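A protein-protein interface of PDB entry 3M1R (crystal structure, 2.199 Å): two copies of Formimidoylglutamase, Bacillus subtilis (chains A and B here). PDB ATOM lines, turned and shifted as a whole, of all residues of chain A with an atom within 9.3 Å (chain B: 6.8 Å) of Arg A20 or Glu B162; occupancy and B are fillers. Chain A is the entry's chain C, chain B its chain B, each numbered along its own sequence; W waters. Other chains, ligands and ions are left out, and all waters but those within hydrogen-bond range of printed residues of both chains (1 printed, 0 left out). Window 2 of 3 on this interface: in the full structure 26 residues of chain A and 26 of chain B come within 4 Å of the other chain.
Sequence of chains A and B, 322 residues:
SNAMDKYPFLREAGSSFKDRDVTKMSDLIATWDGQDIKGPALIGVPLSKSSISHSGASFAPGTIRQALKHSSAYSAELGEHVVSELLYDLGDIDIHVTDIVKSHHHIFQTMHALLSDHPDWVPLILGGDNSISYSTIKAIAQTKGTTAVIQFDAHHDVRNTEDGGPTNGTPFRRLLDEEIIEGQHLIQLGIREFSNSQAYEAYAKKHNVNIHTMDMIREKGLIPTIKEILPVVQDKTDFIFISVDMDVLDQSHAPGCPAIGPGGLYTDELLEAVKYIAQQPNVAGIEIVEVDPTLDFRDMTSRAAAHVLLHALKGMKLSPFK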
ATOM      1  N   PHE A  17       8.916  14.487   9.596  1.00  0.00           N
ATOM      2  CA  PHE A  17       8.515  13.473   8.625  1.00  0.00           C
ATOM      3  C   PHE A  17       7.287  12.749   9.148  1.00  0.00           C
ATOM      4  O   PHE A  17       7.306  12.200  10.244  1.00  0.00           O
ATOM      5  CB  PHE A  17       9.647  12.471   8.367  1.00  0.00           C
ATOM      6  CG  PHE A  17       9.274  11.358   7.420  1.00  0.00           C
ATOM      7  CD1 PHE A  17       8.801  11.638   6.149  1.00  0.00           C
ATOM      8  CD2 PHE A  17       9.413  10.029   7.795  1.00  0.00           C
ATOM      9  CE1 PHE A  17       8.466  10.616   5.276  1.00  0.00           C
ATOM     10  CE2 PHE A  17       9.083   9.002   6.922  1.00  0.00           C
ATOM     11  CZ  PHE A  17       8.614   9.298   5.666  1.00  0.00           C
ATOM     12  N   LYS A  18       6.209  12.764   8.380  1.00  0.00           N
ATOM     13  CA  LYS A  18       5.020  12.048   8.798  1.00  0.00           C
ATOM     14  C   LYS A  18       4.937  10.689   8.102  1.00  0.00           C
ATOM     15  O   LYS A  18       4.959  10.606   6.871  1.00  0.00           O
ATOM     16  CB  LYS A  18       3.761  12.881   8.554  1.00  0.00           C
ATOM     17  CG  LYS A  18       2.710  12.706   9.638  1.00  0.00           C
ATOM     18  CD  LYS A  18       1.762  13.896   9.690  1.00  0.00           C
ATOM     19  CE  LYS A  18       1.051  14.111   8.351  1.00  0.00           C
ATOM     20  NZ  LYS A  18       0.058  15.233   8.389  1.00  0.00           N
ATOM     21  N   ASP A  19       4.884   9.627   8.902  1.00  0.00           N
ATOM     22  CA  ASP A  19       4.683   8.285   8.372  1.00  0.00           C
ATOM     23  C   ASP A  19       3.319   7.798   8.821  1.00  0.00           C
ATOM     24  O   ASP A  19       3.090   7.607  10.016  1.00  0.00           O
ATOM     25  CB  ASP A  19       5.772   7.326   8.856  1.00  0.00           C
ATOM     26  CG  ASP A  19       5.741   5.981   8.126  1.00  0.00           C
ATOM     27  OD1 ASP A  19       4.637   5.436   7.911  1.00  0.00           O
ATOM     28  OD2 ASP A  19       6.819   5.461   7.766  1.00  0.00           O
ATOM     29  N   ARG A  20       2.423   7.608   7.854  1.00  0.00           N
ATOM     30  CA  ARG A  20       1.042   7.194   8.101  1.00  0.00           C
ATOM     31  C   ARG A  20       0.939   5.882   8.868  1.00  0.00           C
ATOM     32  O   ARG A  20       0.006   5.687   9.647  1.00  0.00           O
ATOM     33  CB  ARG A  20       0.288   7.057   6.779  1.00  0.00           C
ATOM     34  CG  ARG A  20       1.099   7.447   5.556  1.00  0.00           C
ATOM     35  CD  ARG A  20       0.291   7.292   4.265  1.00  0.00           C
ATOM     36  NE  ARG A  20       0.384   5.945   3.705  1.00  0.00           N
ATOM     37  CZ  ARG A  20       1.209   5.603   2.722  1.00  0.00           C
ATOM     38  NH1 ARG A  20       2.009   6.510   2.184  1.00  0.00           N
ATOM     39  NH2 ARG A  20       1.231   4.355   2.273  1.00  0.00           N
ATOM     40  N   ASP A  21       1.894   4.985   8.636  1.00  0.00           N
ATOM     41  CA  ASP A  21       1.892   3.659   9.258  1.00  0.00           C
ATOM     42  C   ASP A  21       2.549   3.652  10.638  1.00  0.00           C
ATOM     43  O   ASP A  21       2.734   2.592  11.238  1.00  0.00           O
ATOM     44  CB  ASP A  21       2.597   2.644   8.354  1.00  0.00           C
ATOM     45  CG  ASP A  21       1.858   2.409   7.043  1.00  0.00           C
ATOM     46  OD1 ASP A  21       2.440   2.688   5.972  1.00  0.00           O
ATOM     47  OD2 ASP A  21       0.699   1.943   7.085  1.00  0.00           O
ATOM     48  N   VAL A  22       2.901   4.833  11.140  1.00  0.00           N
ATOM     49  CA  VAL A  22       3.603   4.934  12.417  1.00  0.00           C
ATOM     50  C   VAL A  22       2.825   5.769  13.412  1.00  0.00           C
ATOM     51  O   VAL A  22       2.238   6.791  13.067  1.00  0.00           O
ATOM     52  CB  VAL A  22       4.989   5.570  12.245  1.00  0.00           C
ATOM     53  CG1 VAL A  22       5.628   5.830  13.609  1.00  0.00           C
ATOM     54  CG2 VAL A  22       5.872   4.683  11.385  1.00  0.00           C
ATOM     55  N   THR A  23       2.818   5.329  14.658  1.00  0.00           N
ATOM     56  CA  THR A  23       2.203   6.124  15.700  1.00  0.00           C
ATOM     57  C   THR A  23       3.201   6.423  16.829  1.00  0.00           C
ATOM     58  O   THR A  23       3.583   5.548  17.610  1.00  0.00           O
ATOM     59  CB  THR A  23       0.888   5.487  16.182  1.00  0.00           C
ATOM     60  OG1 THR A  23       0.504   6.051  17.441  1.00  0.00           O
ATOM     61  CG2 THR A  23       1.041   3.984  16.299  1.00  0.00           C
ATOM     62  N   LYS A  24       3.642   7.675  16.867  1.00  0.00           N
ATOM     63  CA  LYS A  24       4.581   8.142  17.871  1.00  0.00           C
ATOM     64  C   LYS A  24       3.825   8.678  19.077  1.00  0.00           C
ATOM     65  O   LYS A  24       2.613   8.899  19.016  1.00  0.00           O
ATOM     66  CB  LYS A  24       5.465   9.242  17.282  1.00  0.00           C
ATOM     67  CG  LYS A  24       6.578   8.728  16.392  1.00  0.00           C
ATOM     68  CD  LYS A  24       7.005   9.765  15.346  1.00  0.00           C
ATOM     69  CE  LYS A  24       7.486  11.073  15.959  1.00  0.00           C
ATOM     70  NZ  LYS A  24       8.039  12.002  14.908  1.00  0.00           N
ATOM     71  N   ASP A  27       1.786  11.692  18.602  1.00  0.00           N
ATOM     72  CA  ASP A  27       0.451  11.551  18.030  1.00  0.00           C
ATOM     73  C   ASP A  27      -0.572  11.293  19.127  1.00  0.00           C
ATOM     74  O   ASP A  27      -1.777  11.375  18.889  1.00  0.00           O
ATOM     75  CB  ASP A  27       0.415  10.410  17.010  1.00  0.00           C
ATOM     76  CG  ASP A  27       1.383  10.633  15.853  1.00  0.00           C
ATOM     77  OD1 ASP A  27       1.503  11.796  15.397  1.00  0.00           O
ATOM     78  OD2 ASP A  27       2.025   9.650  15.402  1.00  0.00           O
ATOM     79  N   HIS A  81      -0.397  -0.354  22.031  1.00  0.00           N
ATOM     80  CA  HIS A  81       0.208   0.907  22.413  1.00  0.00           C
ATOM     81  C   HIS A  81       0.115   1.139  23.921  1.00  0.00           C
ATOM     82  O   HIS A  81      -0.901   0.814  24.542  1.00  0.00           O
ATOM     83  CB  HIS A  81      -0.451   2.022  21.623  1.00  0.00           C
ATOM     84  CG  HIS A  81      -0.304   1.855  20.146  1.00  0.00           C
ATOM     85  ND1 HIS A  81      -1.192   1.124  19.386  1.00  0.00           N
ATOM     86  CD2 HIS A  81       0.648   2.298  19.288  1.00  0.00           C
ATOM     87  CE1 HIS A  81      -0.805   1.142  18.124  1.00  0.00           C
ATOM     88  NE2 HIS A  81       0.310   1.845  18.039  1.00  0.00           N
ATOM     89  N   ARG B 159       9.482   0.113   6.247  1.00  0.00           N
ATOM     90  CA  ARG B 159       8.684   1.319   6.080  1.00  0.00           C
ATOM     91  C   ARG B 159       8.137   1.439   4.660  1.00  0.00           C
ATOM     92  O   ARG B 159       8.834   1.138   3.691  1.00  0.00           O
ATOM     93  CB  ARG B 159       9.523   2.563   6.374  1.00  0.00           C
ATOM     94  CG  ARG B 159       9.849   2.829   7.835  1.00  0.00           C
ATOM     95  CD  ARG B 159      10.341   4.268   7.954  1.00  0.00           C
ATOM     96  NE  ARG B 159      10.694   4.668   9.309  1.00  0.00           N
ATOM     97  CZ  ARG B 159      10.065   5.618   9.994  1.00  0.00           C
ATOM     98  NH1 ARG B 159       9.034   6.254   9.448  1.00  0.00           N
ATOM     99  NH2 ARG B 159      10.470   5.938  11.221  1.00  0.00           N
ATOM    100  N   ASN B 160       6.907   1.920   4.536  1.00  0.00           N
ATOM    101  CA  ASN B 160       6.325   2.161   3.216  1.00  0.00           C
ATOM    102  C   ASN B 160       7.173   3.159   2.416  1.00  0.00           C
ATOM    103  O   ASN B 160       7.907   3.968   2.995  1.00  0.00           O
ATOM    104  CB  ASN B 160       4.873   2.635   3.337  1.00  0.00           C
ATOM    105  CG  ASN B 160       4.765   4.088   3.762  1.00  0.00           C
ATOM    106  OD1 ASN B 160       5.202   4.990   3.047  1.00  0.00           O
ATOM    107  ND2 ASN B 160       4.172   4.322   4.927  1.00  0.00           N
ATOM    108  N   THR B 161       7.074   3.096   1.089  1.00  0.00           N
ATOM    109  CA  THR B 161       7.949   3.872   0.214  1.00  0.00           C
ATOM    110  C   THR B 161       7.322   5.201  -0.235  1.00  0.00           C
ATOM    111  O   THR B 161       8.026   6.101  -0.715  1.00  0.00           O
ATOM    112  CB  THR B 161       8.382   3.035  -1.025  1.00  0.00           C
ATOM    113  OG1 THR B 161       9.230   1.958  -0.608  1.00  0.00           O
ATOM    114  CG2 THR B 161       9.141   3.890  -2.027  1.00  0.00           C
ATOM    115  N   GLU B 162       6.008   5.329  -0.054  1.00  0.00           N
ATOM    116  CA  GLU B 162       5.263   6.495  -0.543  1.00  0.00           C
ATOM    117  C   GLU B 162       5.455   7.800   0.254  1.00  0.00           C
ATOM    118  O   GLU B 162       5.263   8.892  -0.275  1.00  0.00           O
ATOM    119  CB  GLU B 162       3.770   6.164  -0.631  1.00  0.00           C
ATOM    120  CG  GLU B 162       3.453   4.890  -1.402  1.00  0.00           C
ATOM    121  CD  GLU B 162       2.696   3.871  -0.562  1.00  0.00           C
ATOM    122  OE1 GLU B 162       1.552   3.531  -0.936  1.00  0.00           O
ATOM    123  OE2 GLU B 162       3.242   3.415   0.471  1.00  0.00           O
ATOM    124  N   ASP B 163       5.824   7.693   1.524  1.00  0.00           N
ATOM    125  CA  ASP B 163       5.904   8.881   2.377  1.00  0.00           C
ATOM    126  C   ASP B 163       7.180   9.698   2.170  1.00  0.00           C
ATOM    127  O   ASP B 163       7.141  10.927   2.163  1.00  0.00           O
ATOM    128  CB  ASP B 163       5.717   8.502   3.849  1.00  0.00           C
ATOM    129  CG  ASP B 163       4.296   8.054   4.154  1.00  0.00           C
ATOM    130  OD1 ASP B 163       3.362   8.588   3.519  1.00  0.00           O
ATOM    131  OD2 ASP B 163       4.108   7.167   5.017  1.00  0.00           O
ATOM    132  N   GLY B 164       8.303   9.014   1.982  1.00  0.00           N
ATOM    133  CA  GLY B 164       9.581   9.686   1.834  1.00  0.00           C
ATOM    134  C   GLY B 164      10.464   9.167   0.712  1.00  0.00           C
ATOM    135  O   GLY B 164      11.627   9.544   0.628  1.00  0.00           O
ATOM    136  N   GLY B 165       9.922   8.326  -0.166  1.00  0.00           N
ATOM    137  CA  GLY B 165      10.732   7.710  -1.207  1.00  0.00           C
ATOM    138  C   GLY B 165      11.588   6.579  -0.641  1.00  0.00           C
ATOM    139  O   GLY B 165      11.291   6.076   0.444  1.00  0.00           O
ATOM    140  N   THR B 170      13.180   2.015   4.372  1.00  0.00           N
ATOM    141  CA  THR B 170      12.423   1.163   3.438  1.00  0.00           C
ATOM    142  C   THR B 170      13.102  -0.056   2.814  1.00  0.00           C
ATOM    143  O   THR B 170      12.445  -0.797   2.091  1.00  0.00           O
ATOM    144  CB  THR B 170      11.996   1.952   2.198  1.00  0.00           C
ATOM    145  OG1 THR B 170      13.170   2.276   1.430  1.00  0.00           O
ATOM    146  CG2 THR B 170      11.240   3.226   2.577  1.00  0.00           C
ATOM    147  N   ARG B 173      11.311  -3.526   2.924  1.00  0.00           N
ATOM    148  CA  ARG B 173      10.048  -3.435   2.204  1.00  0.00           C
ATOM    149  C   ARG B 173      10.311  -3.665   0.715  1.00  0.00           C
ATOM    150  O   ARG B 173       9.780  -4.598   0.109  1.00  0.00           O
ATOM    151  CB  ARG B 173       9.443  -2.045   2.383  1.00  0.00           C
ATOM    152  CG  ARG B 173       8.039  -1.887   1.834  1.00  0.00           C
ATOM    153  CD  ARG B 173       7.053  -2.354   2.875  1.00  0.00           C
ATOM    154  NE  ARG B 173       5.813  -1.601   2.806  1.00  0.00           N
ATOM    155  CZ  ARG B 173       5.020  -1.371   3.845  1.00  0.00           C
ATOM    156  NH1 ARG B 173       3.905  -0.674   3.682  1.00  0.00           N
ATOM    157  NH2 ARG B 173       5.342  -1.829   5.042  1.00  0.00           N
ATOM    158  N   ALA B 199       2.130  -1.518  12.615  1.00  0.00           N
ATOM    159  CA  ALA B 199       1.859  -1.877  11.223  1.00  0.00           C
ATOM    160  C   ALA B 199       3.058  -2.539  10.546  1.00  0.00           C
ATOM    161  O   ALA B 199       2.887  -3.389   9.668  1.00  0.00           O
ATOM    162  CB  ALA B 199       1.405  -0.657  10.425  1.00  0.00           C
ATOM    163  N   TYR B 200       4.268  -2.144  10.941  1.00  0.00           N
ATOM    164  CA  TYR B 200       5.467  -2.676  10.295  1.00  0.00           C
ATOM    165  C   TYR B 200       5.856  -4.049  10.819  1.00  0.00           C
ATOM    166  O   TYR B 200       6.315  -4.902  10.067  1.00  0.00           O
ATOM    167  CB  TYR B 200       6.628  -1.697  10.399  1.00  0.00           C
ATOM    168  CG  TYR B 200       6.397  -0.451   9.583  1.00  0.00           C
ATOM    169  CD1 TYR B 200       5.714  -0.512   8.377  1.00  0.00           C
ATOM    170  CD2 TYR B 200       6.846   0.781  10.019  1.00  0.00           C
ATOM    171  CE1 TYR B 200       5.495   0.628   7.612  1.00  0.00           C
ATOM    172  CE2 TYR B 200       6.627   1.937   9.261  1.00  0.00           C
ATOM    173  CZ  TYR B 200       5.954   1.848   8.061  1.00  0.00           C
ATOM    174  OH  TYR B 200       5.738   2.977   7.305  1.00  0.00           O
HETATM  175  O   HOH W   1       7.891   5.908   5.583  1.00  0.00           O
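Water W1 bridges OD2 of Asp A19 (2.5 Å) and O of Asn B160 (3.2 Å).
Among the printed residues, pairs that only touch across the chains: Phe A17 with Arg B159 (3.7 Å), Phe A17 with Asp B163 (3.4 Å), Phe A17 with Gly B164 (3.7 Å), Lys A18 with Asp B163 (3.8 Å), Arg A20 with Asn B160 (3.6 Å), Asp A21 with Ala B199 (3.6 Å), Asp A21 with Tyr B200 (3.3 Å) and Val A22 with Tyr B200 (3.6 Å).
The guanidinium group (NH1) of Arg B159 lies within salt-bridge range of the side-chain carboxylate (OD2) of Asp A19 (2.9 Å).
The side-chain amide nitrogen (ND2) of Asn B160 sits at hydrogen-bond distance from the side-chain carboxylate (OD1) of Asp A19.
The side-chain amide nitrogen (ND2) of Asn B160 lies within hydrogen-bond range of the side-chain carboxylate (OD1) of Asp A21 (2.6 Å).
The guanidinium group (NH2) of Arg A20 is in salt-bridge range of the side-chain carboxylate (OE2) of Glu B162 (2.9 Å).
The side-chain carboxylate of Asp B163 is in salt-bridge range of the guanidinium group of Arg A20 (2.8 Å).
The side-chain carboxylate (OD2) of Asp A19 lies within hydrogen-bond range of the side-chain hydroxyl (OH) of Tyr B200, 2.7 Å away.
OD1 of Asp A19 sits close to OD2 of Asp B163 (3.4 Å).
Hydrophobic or aromatic side chains of chain B within 4 Å of the printed part of chain A: Ala B199 and Tyr B200.
Of the 10 printed residues of chain A, 6 touch a printed residue of chain B.
Among the printed residues, Asp or Glu carboxylates within 4 Å of a Lys or Arg side-chain nitrogen of the other chain: Asp A19 with Arg B159, Arg A20 with Glu B162 and Arg A20 with Asp B163.
N of Glu B162 lies within hydrogen-bond range of OD1 of Asn B160 (3.2 Å).
OD2 of Asp B163 sits at hydrogen-bond distance from ND2 of Asn B160 (2.8 Å).
The side-chain hydroxyl (OH) of Tyr B200 is in hydrogen-bond range of the side-chain amide nitrogen (ND2) of Asn B160.
The side-chain carboxylate (OD1) of Asp A19 is in hydrogen-bond range of the backbone NH (N) of Asp A21 (2.9 Å).
No position is printed for both chains.
Of the 15 pairs that touch across the chains among the printed residues, none has its exchanged pair printed and touching as well.
Of the printed residues of chain B, Phe A17 touches Arg B159 (3.7 Å), Asp B163 (3.4 Å) and Gly B164 (3.7 Å).
Printed residues of chain B within 4 Å of Lys A18: Asp B163 (3.8 Å).
Arg A20 touches just these residues of chain B: Asn B160, Glu B162 and Asp B163.
Asp A27 touches none of the printed residues of chain B.
Of the printed residues of chain A, Asn B160 touches Asp A19, Arg A20 and Asp A21.
No residue of chain A comes within 4 Å of Thr B161.
Glu B162 touches one residue of chain A.
Of the printed residues of chain A, Asp B163 touches Phe A17 (3.4 Å), Lys A18 (3.8 Å), Asp A19 (3.4 Å) and Arg A20 (2.8 Å).
Of the printed residues of chain A, Ala B199 touches Asp A21 (3.6 Å).
The nearest residue of chain B that does not touch Arg A20 is Tyr B200 (5.7 Å).
The nearest residue of chain A that does not touch Glu B162 is Asp A21 (5.6 Å).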
